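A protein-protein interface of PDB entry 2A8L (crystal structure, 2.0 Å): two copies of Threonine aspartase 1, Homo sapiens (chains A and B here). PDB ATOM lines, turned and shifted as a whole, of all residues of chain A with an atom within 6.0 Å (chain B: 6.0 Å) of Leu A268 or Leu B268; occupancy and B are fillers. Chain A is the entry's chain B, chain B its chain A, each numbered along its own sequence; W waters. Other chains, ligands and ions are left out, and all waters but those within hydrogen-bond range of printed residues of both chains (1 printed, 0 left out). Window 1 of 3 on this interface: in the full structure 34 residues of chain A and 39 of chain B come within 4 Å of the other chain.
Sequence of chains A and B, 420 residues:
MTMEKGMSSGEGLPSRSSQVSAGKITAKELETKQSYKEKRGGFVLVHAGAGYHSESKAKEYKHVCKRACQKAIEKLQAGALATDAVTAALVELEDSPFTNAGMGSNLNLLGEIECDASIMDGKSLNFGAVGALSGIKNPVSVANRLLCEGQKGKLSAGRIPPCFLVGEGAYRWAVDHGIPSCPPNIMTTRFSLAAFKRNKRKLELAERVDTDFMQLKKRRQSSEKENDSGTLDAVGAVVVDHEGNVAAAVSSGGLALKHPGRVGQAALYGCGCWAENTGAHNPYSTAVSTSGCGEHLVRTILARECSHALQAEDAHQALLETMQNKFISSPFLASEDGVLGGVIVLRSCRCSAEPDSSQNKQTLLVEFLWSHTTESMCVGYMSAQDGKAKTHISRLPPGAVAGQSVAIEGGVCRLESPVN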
ATOM      1  N   SER A 118      19.089  11.506   6.536  1.00  0.00           N
ATOM      2  CA  SER A 118      19.921  12.424   7.288  1.00  0.00           C
ATOM      3  C   SER A 118      21.378  12.133   6.999  1.00  0.00           C
ATOM      4  O   SER A 118      21.735  11.060   6.509  1.00  0.00           O
ATOM      5  CB  SER A 118      19.649  12.283   8.791  1.00  0.00           C
ATOM      6  OG  SER A 118      19.881  10.954   9.227  1.00  0.00           O
ATOM      7  N   PHE A 127      24.751  18.746  10.887  1.00  0.00           N
ATOM      8  CA  PHE A 127      23.775  17.717  10.552  1.00  0.00           C
ATOM      9  C   PHE A 127      22.665  18.261   9.663  1.00  0.00           C
ATOM     10  O   PHE A 127      22.296  19.425   9.768  1.00  0.00           O
ATOM     11  CB  PHE A 127      23.183  17.207  11.873  1.00  0.00           C
ATOM     12  CG  PHE A 127      22.015  16.262  11.726  1.00  0.00           C
ATOM     13  CD1 PHE A 127      22.222  14.900  11.530  1.00  0.00           C
ATOM     14  CD2 PHE A 127      20.709  16.726  11.849  1.00  0.00           C
ATOM     15  CE1 PHE A 127      21.149  14.016  11.464  1.00  0.00           C
ATOM     16  CE2 PHE A 127      19.626  15.852  11.784  1.00  0.00           C
ATOM     17  CZ  PHE A 127      19.846  14.492  11.593  1.00  0.00           C
ATOM     18  N   ALA A 129      18.785  16.859   7.837  1.00  0.00           N
ATOM     19  CA  ALA A 129      17.823  15.763   7.780  1.00  0.00           C
ATOM     20  C   ALA A 129      16.470  16.172   7.226  1.00  0.00           C
ATOM     21  O   ALA A 129      16.056  17.323   7.350  1.00  0.00           O
ATOM     22  CB  ALA A 129      17.633  15.180   9.161  1.00  0.00           C
ATOM     23  N   PHE A 164      16.551  20.352  10.207  1.00  0.00           N
ATOM     24  CA  PHE A 164      15.547  19.307  10.032  1.00  0.00           C
ATOM     25  C   PHE A 164      14.231  19.848   9.492  1.00  0.00           C
ATOM     26  O   PHE A 164      13.540  20.617  10.167  1.00  0.00           O
ATOM     27  CB  PHE A 164      15.331  18.593  11.375  1.00  0.00           C
ATOM     28  CG  PHE A 164      14.348  17.446  11.320  1.00  0.00           C
ATOM     29  CD1 PHE A 164      14.244  16.647  10.183  1.00  0.00           C
ATOM     30  CD2 PHE A 164      13.565  17.136  12.436  1.00  0.00           C
ATOM     31  CE1 PHE A 164      13.376  15.555  10.150  1.00  0.00           C
ATOM     32  CE2 PHE A 164      12.697  16.047  12.416  1.00  0.00           C
ATOM     33  CZ  PHE A 164      12.603  15.255  11.266  1.00  0.00           C
ATOM     34  N   VAL A 263       7.326   9.511  10.855  1.00  0.00           N
ATOM     35  CA  VAL A 263       8.762   9.682  10.607  1.00  0.00           C
ATOM     36  C   VAL A 263       9.572   8.701  11.440  1.00  0.00           C
ATOM     37  O   VAL A 263       9.336   8.555  12.637  1.00  0.00           O
ATOM     38  CB  VAL A 263       9.205  11.123  10.942  1.00  0.00           C
ATOM     39  CG1 VAL A 263      10.731  11.262  10.807  1.00  0.00           C
ATOM     40  CG2 VAL A 263       8.488  12.099  10.014  1.00  0.00           C
ATOM     41  N   GLY A 264      10.534   8.044  10.794  1.00  0.00           N
ATOM     42  CA  GLY A 264      11.361   7.062  11.473  1.00  0.00           C
ATOM     43  C   GLY A 264      12.769   7.500  11.830  1.00  0.00           C
ATOM     44  O   GLY A 264      13.124   8.677  11.721  1.00  0.00           O
ATOM     45  N   GLN A 265      13.588   6.533  12.230  1.00  0.00           N
ATOM     46  CA  GLN A 265      14.952   6.815  12.662  1.00  0.00           C
ATOM     47  C   GLN A 265      15.917   7.400  11.638  1.00  0.00           C
ATOM     48  O   GLN A 265      16.899   8.026  12.027  1.00  0.00           O
ATOM     49  CB  GLN A 265      15.582   5.554  13.278  1.00  0.00           C
ATOM     50  CG  GLN A 265      16.506   4.771  12.356  1.00  0.00           C
ATOM     51  CD  GLN A 265      15.769   4.106  11.221  1.00  0.00           C
ATOM     52  OE1 GLN A 265      14.560   3.902  11.292  1.00  0.00           O
ATOM     53  NE2 GLN A 265      16.497   3.744  10.170  1.00  0.00           N
ATOM     54  N   ALA A 266      15.653   7.201  10.346  1.00  0.00           N
ATOM     55  CA  ALA A 266      16.547   7.717   9.307  1.00  0.00           C
ATOM     56  C   ALA A 266      16.542   9.250   9.237  1.00  0.00           C
ATOM     57  O   ALA A 266      17.445   9.861   8.654  1.00  0.00           O
ATOM     58  CB  ALA A 266      16.168   7.122   7.942  1.00  0.00           C
ATOM     59  N   ALA A 267      15.528   9.861   9.844  1.00  0.00           N
ATOM     60  CA  ALA A 267      15.394  11.319   9.857  1.00  0.00           C
ATOM     61  C   ALA A 267      15.736  11.937  11.214  1.00  0.00           C
ATOM     62  O   ALA A 267      15.838  13.162  11.335  1.00  0.00           O
ATOM     63  CB  ALA A 267      13.948  11.714   9.486  1.00  0.00           C
ATOM     64  N   LEU A 268      15.914  11.098  12.229  1.00  0.00           N
ATOM     65  CA  LEU A 268      16.160  11.594  13.576  1.00  0.00           C
ATOM     66  C   LEU A 268      17.607  11.644  14.063  1.00  0.00           C
ATOM     67  O   LEU A 268      18.304  10.624  14.099  1.00  0.00           O
ATOM     68  CB  LEU A 268      15.322  10.784  14.570  1.00  0.00           C
ATOM     69  CG  LEU A 268      13.803  10.803  14.325  1.00  0.00           C
ATOM     70  CD1 LEU A 268      13.081  10.057  15.431  1.00  0.00           C
ATOM     71  CD2 LEU A 268      13.316  12.234  14.283  1.00  0.00           C
ATOM     72  N   TYR A 269      18.021  12.844  14.467  1.00  0.00           N
ATOM     73  CA  TYR A 269      19.370  13.110  14.985  1.00  0.00           C
ATOM     74  C   TYR A 269      19.779  12.091  16.047  1.00  0.00           C
ATOM     75  O   TYR A 269      19.023  11.821  16.990  1.00  0.00           O
ATOM     76  CB  TYR A 269      19.419  14.518  15.599  1.00  0.00           C
ATOM     77  CG  TYR A 269      20.798  14.993  16.024  1.00  0.00           C
ATOM     78  CD1 TYR A 269      21.758  15.345  15.081  1.00  0.00           C
ATOM     79  CD2 TYR A 269      21.116  15.150  17.375  1.00  0.00           C
ATOM     80  CE1 TYR A 269      23.007  15.852  15.468  1.00  0.00           C
ATOM     81  CE2 TYR A 269      22.360  15.657  17.775  1.00  0.00           C
ATOM     82  CZ  TYR A 269      23.299  16.008  16.816  1.00  0.00           C
ATOM     83  OH  TYR A 269      24.515  16.536  17.207  1.00  0.00           O
ATOM     84  N   GLY A 270      20.973  11.531  15.890  1.00  0.00           N
ATOM     85  CA  GLY A 270      21.476  10.561  16.847  1.00  0.00           C
ATOM     86  C   GLY A 270      20.925   9.150  16.722  1.00  0.00           C
ATOM     87  O   GLY A 270      21.460   8.220  17.322  1.00  0.00           O
ATOM     88  N   CYS A 271      19.862   8.980  15.942  1.00  0.00           N
ATOM     89  CA  CYS A 271      19.245   7.667  15.771  1.00  0.00           C
ATOM     90  C   CYS A 271      19.632   6.963  14.470  1.00  0.00           C
ATOM     91  O   CYS A 271      20.040   5.796  14.484  1.00  0.00           O
ATOM     92  CB  CYS A 271      17.715   7.804  15.844  1.00  0.00           C
ATOM     93  SG  CYS A 271      17.127   8.635  17.336  1.00  0.00           S
ATOM     94  N   GLY A 272      19.506   7.674  13.351  1.00  0.00           N
ATOM     95  CA  GLY A 272      19.820   7.095  12.056  1.00  0.00           C
ATOM     96  C   GLY A 272      21.296   7.057  11.705  1.00  0.00           C
ATOM     97  O   GLY A 272      21.769   6.095  11.102  1.00  0.00           O
ATOM     98  N   CYS A 273      22.034   8.098  12.068  1.00  0.00           N
ATOM     99  CA  CYS A 273      23.461   8.112  11.763  1.00  0.00           C
ATOM    100  C   CYS A 273      24.198   9.021  12.713  1.00  0.00           C
ATOM    101  O   CYS A 273      23.587   9.767  13.479  1.00  0.00           O
ATOM    102  CB  CYS A 273      23.699   8.572  10.316  1.00  0.00           C
ATOM    103  SG  CYS A 273      23.322  10.335   9.946  1.00  0.00           S
ATOM    104  N   VAL A 298      15.134   4.394  17.381  1.00  0.00           N
ATOM    105  CA  VAL A 298      14.880   5.711  17.968  1.00  0.00           C
ATOM    106  C   VAL A 298      14.887   5.686  19.494  1.00  0.00           C
ATOM    107  O   VAL A 298      15.565   6.496  20.139  1.00  0.00           O
ATOM    108  CB  VAL A 298      13.514   6.273  17.551  1.00  0.00           C
ATOM    109  CG1 VAL A 298      13.261   7.588  18.289  1.00  0.00           C
ATOM    110  CG2 VAL A 298      13.457   6.467  16.044  1.00  0.00           C
ATOM    111  N   SER B 118       5.918  17.158  22.473  1.00  0.00           N
ATOM    112  CA  SER B 118       6.189  15.774  22.822  1.00  0.00           C
ATOM    113  C   SER B 118       5.976  15.585  24.312  1.00  0.00           C
ATOM    114  O   SER B 118       5.923  16.552  25.072  1.00  0.00           O
ATOM    115  CB  SER B 118       7.625  15.385  22.432  1.00  0.00           C
ATOM    116  OG  SER B 118       8.556  16.267  23.025  1.00  0.00           O
ATOM    117  N   PHE B 127       6.658   7.266  24.685  1.00  0.00           N
ATOM    118  CA  PHE B 127       6.806   8.629  24.205  1.00  0.00           C
ATOM    119  C   PHE B 127       5.788   8.919  23.108  1.00  0.00           C
ATOM    120  O   PHE B 127       5.367   8.011  22.400  1.00  0.00           O
ATOM    121  CB  PHE B 127       8.244   8.726  23.664  1.00  0.00           C
ATOM    122  CG  PHE B 127       8.590  10.017  22.995  1.00  0.00           C
ATOM    123  CD1 PHE B 127       8.975  11.129  23.743  1.00  0.00           C
ATOM    124  CD2 PHE B 127       8.610  10.103  21.603  1.00  0.00           C
ATOM    125  CE1 PHE B 127       9.384  12.308  23.108  1.00  0.00           C
ATOM    126  CE2 PHE B 127       9.016  11.283  20.961  1.00  0.00           C
ATOM    127  CZ  PHE B 127       9.402  12.382  21.716  1.00  0.00           C
ATOM    128  N   ALA B 129       4.832  12.226  20.147  1.00  0.00           N
ATOM    129  CA  ALA B 129       5.268  13.509  19.590  1.00  0.00           C
ATOM    130  C   ALA B 129       4.662  13.863  18.237  1.00  0.00           C
ATOM    131  O   ALA B 129       4.302  12.989  17.448  1.00  0.00           O
ATOM    132  CB  ALA B 129       6.804  13.529  19.467  1.00  0.00           C
ATOM    133  N   PHE B 164       5.660   9.234  16.594  1.00  0.00           N
ATOM    134  CA  PHE B 164       6.002  10.549  16.053  1.00  0.00           C
ATOM    135  C   PHE B 164       5.376  10.782  14.684  1.00  0.00           C
ATOM    136  O   PHE B 164       5.719  10.111  13.714  1.00  0.00           O
ATOM    137  CB  PHE B 164       7.535  10.689  15.965  1.00  0.00           C
ATOM    138  CG  PHE B 164       8.011  11.999  15.382  1.00  0.00           C
ATOM    139  CD1 PHE B 164       7.337  13.191  15.647  1.00  0.00           C
ATOM    140  CD2 PHE B 164       9.171  12.049  14.616  1.00  0.00           C
ATOM    141  CE1 PHE B 164       7.816  14.412  15.162  1.00  0.00           C
ATOM    142  CE2 PHE B 164       9.659  13.263  14.125  1.00  0.00           C
ATOM    143  CZ  PHE B 164       8.983  14.445  14.398  1.00  0.00           C
ATOM    144  N   VAL B 263      11.391  21.699  11.917  1.00  0.00           N
ATOM    145  CA  VAL B 263      11.067  21.082  13.192  1.00  0.00           C
ATOM    146  C   VAL B 263      12.174  21.311  14.210  1.00  0.00           C
ATOM    147  O   VAL B 263      13.360  21.191  13.885  1.00  0.00           O
ATOM    148  CB  VAL B 263      10.813  19.571  12.998  1.00  0.00           C
ATOM    149  CG1 VAL B 263      10.434  18.911  14.322  1.00  0.00           C
ATOM    150  CG2 VAL B 263       9.698  19.379  11.968  1.00  0.00           C
ATOM    151  N   GLY B 264      11.773  21.654  15.436  1.00  0.00           N
ATOM    152  CA  GLY B 264      12.722  21.911  16.510  1.00  0.00           C
ATOM    153  C   GLY B 264      12.784  20.826  17.573  1.00  0.00           C
ATOM    154  O   GLY B 264      12.269  19.728  17.375  1.00  0.00           O
ATOM    155  N   GLN B 265      13.384  21.141  18.719  1.00  0.00           N
ATOM    156  CA  GLN B 265      13.535  20.158  19.791  1.00  0.00           C
ATOM    157  C   GLN B 265      12.255  19.678  20.478  1.00  0.00           C
ATOM    158  O   GLN B 265      12.253  18.596  21.053  1.00  0.00           O
ATOM    159  CB  GLN B 265      14.507  20.680  20.865  1.00  0.00           C
ATOM    160  CG  GLN B 265      13.875  21.343  22.096  1.00  0.00           C
ATOM    161  CD  GLN B 265      13.120  22.629  21.788  1.00  0.00           C
ATOM    162  OE1 GLN B 265      13.189  23.153  20.680  1.00  0.00           O
ATOM    163  NE2 GLN B 265      12.394  23.143  22.780  1.00  0.00           N
ATOM    164  N   ALA B 266      11.176  20.453  20.430  1.00  0.00           N
ATOM    165  CA  ALA B 266       9.939  20.033  21.109  1.00  0.00           C
ATOM    166  C   ALA B 266       9.288  18.775  20.519  1.00  0.00           C
ATOM    167  O   ALA B 266       8.426  18.169  21.155  1.00  0.00           O
ATOM    168  CB  ALA B 266       8.909  21.199  21.146  1.00  0.00           C
ATOM    169  N   ALA B 267       9.700  18.377  19.318  1.00  0.00           N
ATOM    170  CA  ALA B 267       9.134  17.192  18.672  1.00  0.00           C
ATOM    171  C   ALA B 267      10.089  16.005  18.649  1.00  0.00           C
ATOM    172  O   ALA B 267       9.687  14.891  18.314  1.00  0.00           O
ATOM    173  CB  ALA B 267       8.717  17.524  17.229  1.00  0.00           C
ATOM    174  N   LEU B 268      11.344  16.239  19.019  1.00  0.00           N
ATOM    175  CA  LEU B 268      12.360  15.193  18.970  1.00  0.00           C
ATOM    176  C   LEU B 268      12.693  14.483  20.263  1.00  0.00           C
ATOM    177  O   LEU B 268      12.955  15.104  21.296  1.00  0.00           O
ATOM    178  CB  LEU B 268      13.661  15.759  18.382  1.00  0.00           C
ATOM    179  CG  LEU B 268      13.549  16.370  16.983  1.00  0.00           C
ATOM    180  CD1 LEU B 268      14.923  16.810  16.502  1.00  0.00           C
ATOM    181  CD2 LEU B 268      12.952  15.361  16.031  1.00  0.00           C
ATOM    182  N   TYR B 269      12.709  13.161  20.170  1.00  0.00           N
ATOM    183  CA  TYR B 269      13.021  12.279  21.281  1.00  0.00           C
ATOM    184  C   TYR B 269      14.396  12.636  21.853  1.00  0.00           C
ATOM    185  O   TYR B 269      15.343  12.892  21.096  1.00  0.00           O
ATOM    186  CB  TYR B 269      13.033  10.843  20.762  1.00  0.00           C
ATOM    187  CG  TYR B 269      13.206   9.773  21.811  1.00  0.00           C
ATOM    188  CD1 TYR B 269      12.180   9.474  22.708  1.00  0.00           C
ATOM    189  CD2 TYR B 269      14.380   9.018  21.871  1.00  0.00           C
ATOM    190  CE1 TYR B 269      12.312   8.448  23.632  1.00  0.00           C
ATOM    191  CE2 TYR B 269      14.525   7.986  22.794  1.00  0.00           C
ATOM    192  CZ  TYR B 269      13.484   7.705  23.668  1.00  0.00           C
ATOM    193  OH  TYR B 269      13.601   6.662  24.552  1.00  0.00           O
ATOM    194  N   GLY B 270      14.489  12.657  23.181  1.00  0.00           N
ATOM    195  CA  GLY B 270      15.739  12.960  23.858  1.00  0.00           C
ATOM    196  C   GLY B 270      16.200  14.407  23.821  1.00  0.00           C
ATOM    197  O   GLY B 270      17.167  14.768  24.494  1.00  0.00           O
ATOM    198  N   CYS B 271      15.503  15.242  23.057  1.00  0.00           N
ATOM    199  CA  CYS B 271      15.882  16.644  22.920  1.00  0.00           C
ATOM    200  C   CYS B 271      14.968  17.606  23.662  1.00  0.00           C
ATOM    201  O   CYS B 271      15.447  18.427  24.451  1.00  0.00           O
ATOM    202  CB  CYS B 271      15.931  17.015  21.432  1.00  0.00           C
ATOM    203  SG  CYS B 271      17.036  15.944  20.457  1.00  0.00           S
ATOM    204  N   GLY B 272      13.657  17.495  23.420  1.00  0.00           N
ATOM    205  CA  GLY B 272      12.697  18.379  24.060  1.00  0.00           C
ATOM    206  C   GLY B 272      12.327  18.051  25.491  1.00  0.00           C
ATOM    207  O   GLY B 272      12.167  18.956  26.306  1.00  0.00           O
ATOM    208  N   CYS B 273      12.167  16.767  25.809  1.00  0.00           N
ATOM    209  CA  CYS B 273      11.828  16.379  27.170  1.00  0.00           C
ATOM    210  C   CYS B 273      12.312  14.963  27.426  1.00  0.00           C
ATOM    211  O   CYS B 273      12.704  14.266  26.496  1.00  0.00           O
ATOM    212  CB  CYS B 273      10.305  16.469  27.396  1.00  0.00           C
ATOM    213  SG  CYS B 273       9.334  15.233  26.516  1.00  0.00           S
ATOM    214  N   VAL B 298      18.595  20.474  20.059  1.00  0.00           N
ATOM    215  CA  VAL B 298      18.631  19.211  19.320  1.00  0.00           C
ATOM    216  C   VAL B 298      20.062  18.655  19.182  1.00  0.00           C
ATOM    217  O   VAL B 298      20.343  17.507  19.538  1.00  0.00           O
ATOM    218  CB  VAL B 298      18.027  19.388  17.912  1.00  0.00           C
ATOM    219  CG1 VAL B 298      18.285  18.142  17.064  1.00  0.00           C
ATOM    220  CG2 VAL B 298      16.532  19.645  18.025  1.00  0.00           C
HETATM  221  O   HOH W   1      15.698  22.261  12.145  1.00  0.00           O
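Ala A129 touches none of the printed residues of chain B. Printed residues of chain B within 4 Å of Val A263: Phe B164 (3.3 Å). Leu A268 touches two residues of chain B. Of the printed residues of chain A, Phe B164 touches Val A263 and Leu A268. Ala B267 touches none of the printed residues of chain A. The nearest residue of chain B that does not touch Leu A268 is Tyr B269 (5.4 Å). The nearest residue of chain A that does not touch Leu B268 is Tyr A269 (5.1 Å). The nearest printed residue of chain A that does not touch Val B263 is Leu A268 (7.3 Å).
Phe A164 touches Leu B268 (CE2 to CD2, 3.7 Å). CE2 of Phe B164 touches CD2 of Leu A268 (3.8 Å). Leu A268 touches Leu B268. O of Val B298 touches CE2 of Tyr A269 (3.3 Å). Tyr B269 touches Val A298.
O of Phe B164 lies within hydrogen-bond range of N of Val A263 (3.3 Å). N of Val B263 is in hydrogen-bond range of O of Phe A164, 3.0 Å away.
The side-chain sulfur of Cys B271 lies within hydrogen-bond range of the backbone carbonyl oxygen of Val B298 (3.8 Å). The side-chain sulfur (SG) of Cys B271 is in hydrogen-bond range of the backbone carbonyl oxygen (O) of Tyr B269 (3.5 Å). SG of Cys A271 lies within hydrogen-bond range of O of Tyr A269 (3.7 Å).
Water W1 bridges the backbone NH (N) of Phe A164 and the backbone carbonyl oxygen (O) of Val B263.
Hydrophobic or aromatic side chains of chain B within 4 Å of the printed part of chain A: Phe B164, Val B263, Leu B268 and Tyr B269. Hydrophobic or aromatic side chains of chain A within 4 Å of the printed part of chain B: Phe A164, Val A263, Leu A268 and Tyr A269. Among the printed residues, 7 pairs touch across the chains.
Phe A164 touches Val B263, and with the chains exchanged Val A263 touches Phe B164. Phe A164 touches Leu B268, and with the chains exchanged Leu A268 touches Phe B164. Leu A268 touches its own counterpart, Leu B268. Tyr A269 touches Val B298, and with the chains exchanged Val A298 touches Tyr B269. Positions printed for both chains: 118, 127, 129, 164, 263, 264, 265, 266, 267, 268, 269, 270, 271, 272, 273 and 298.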
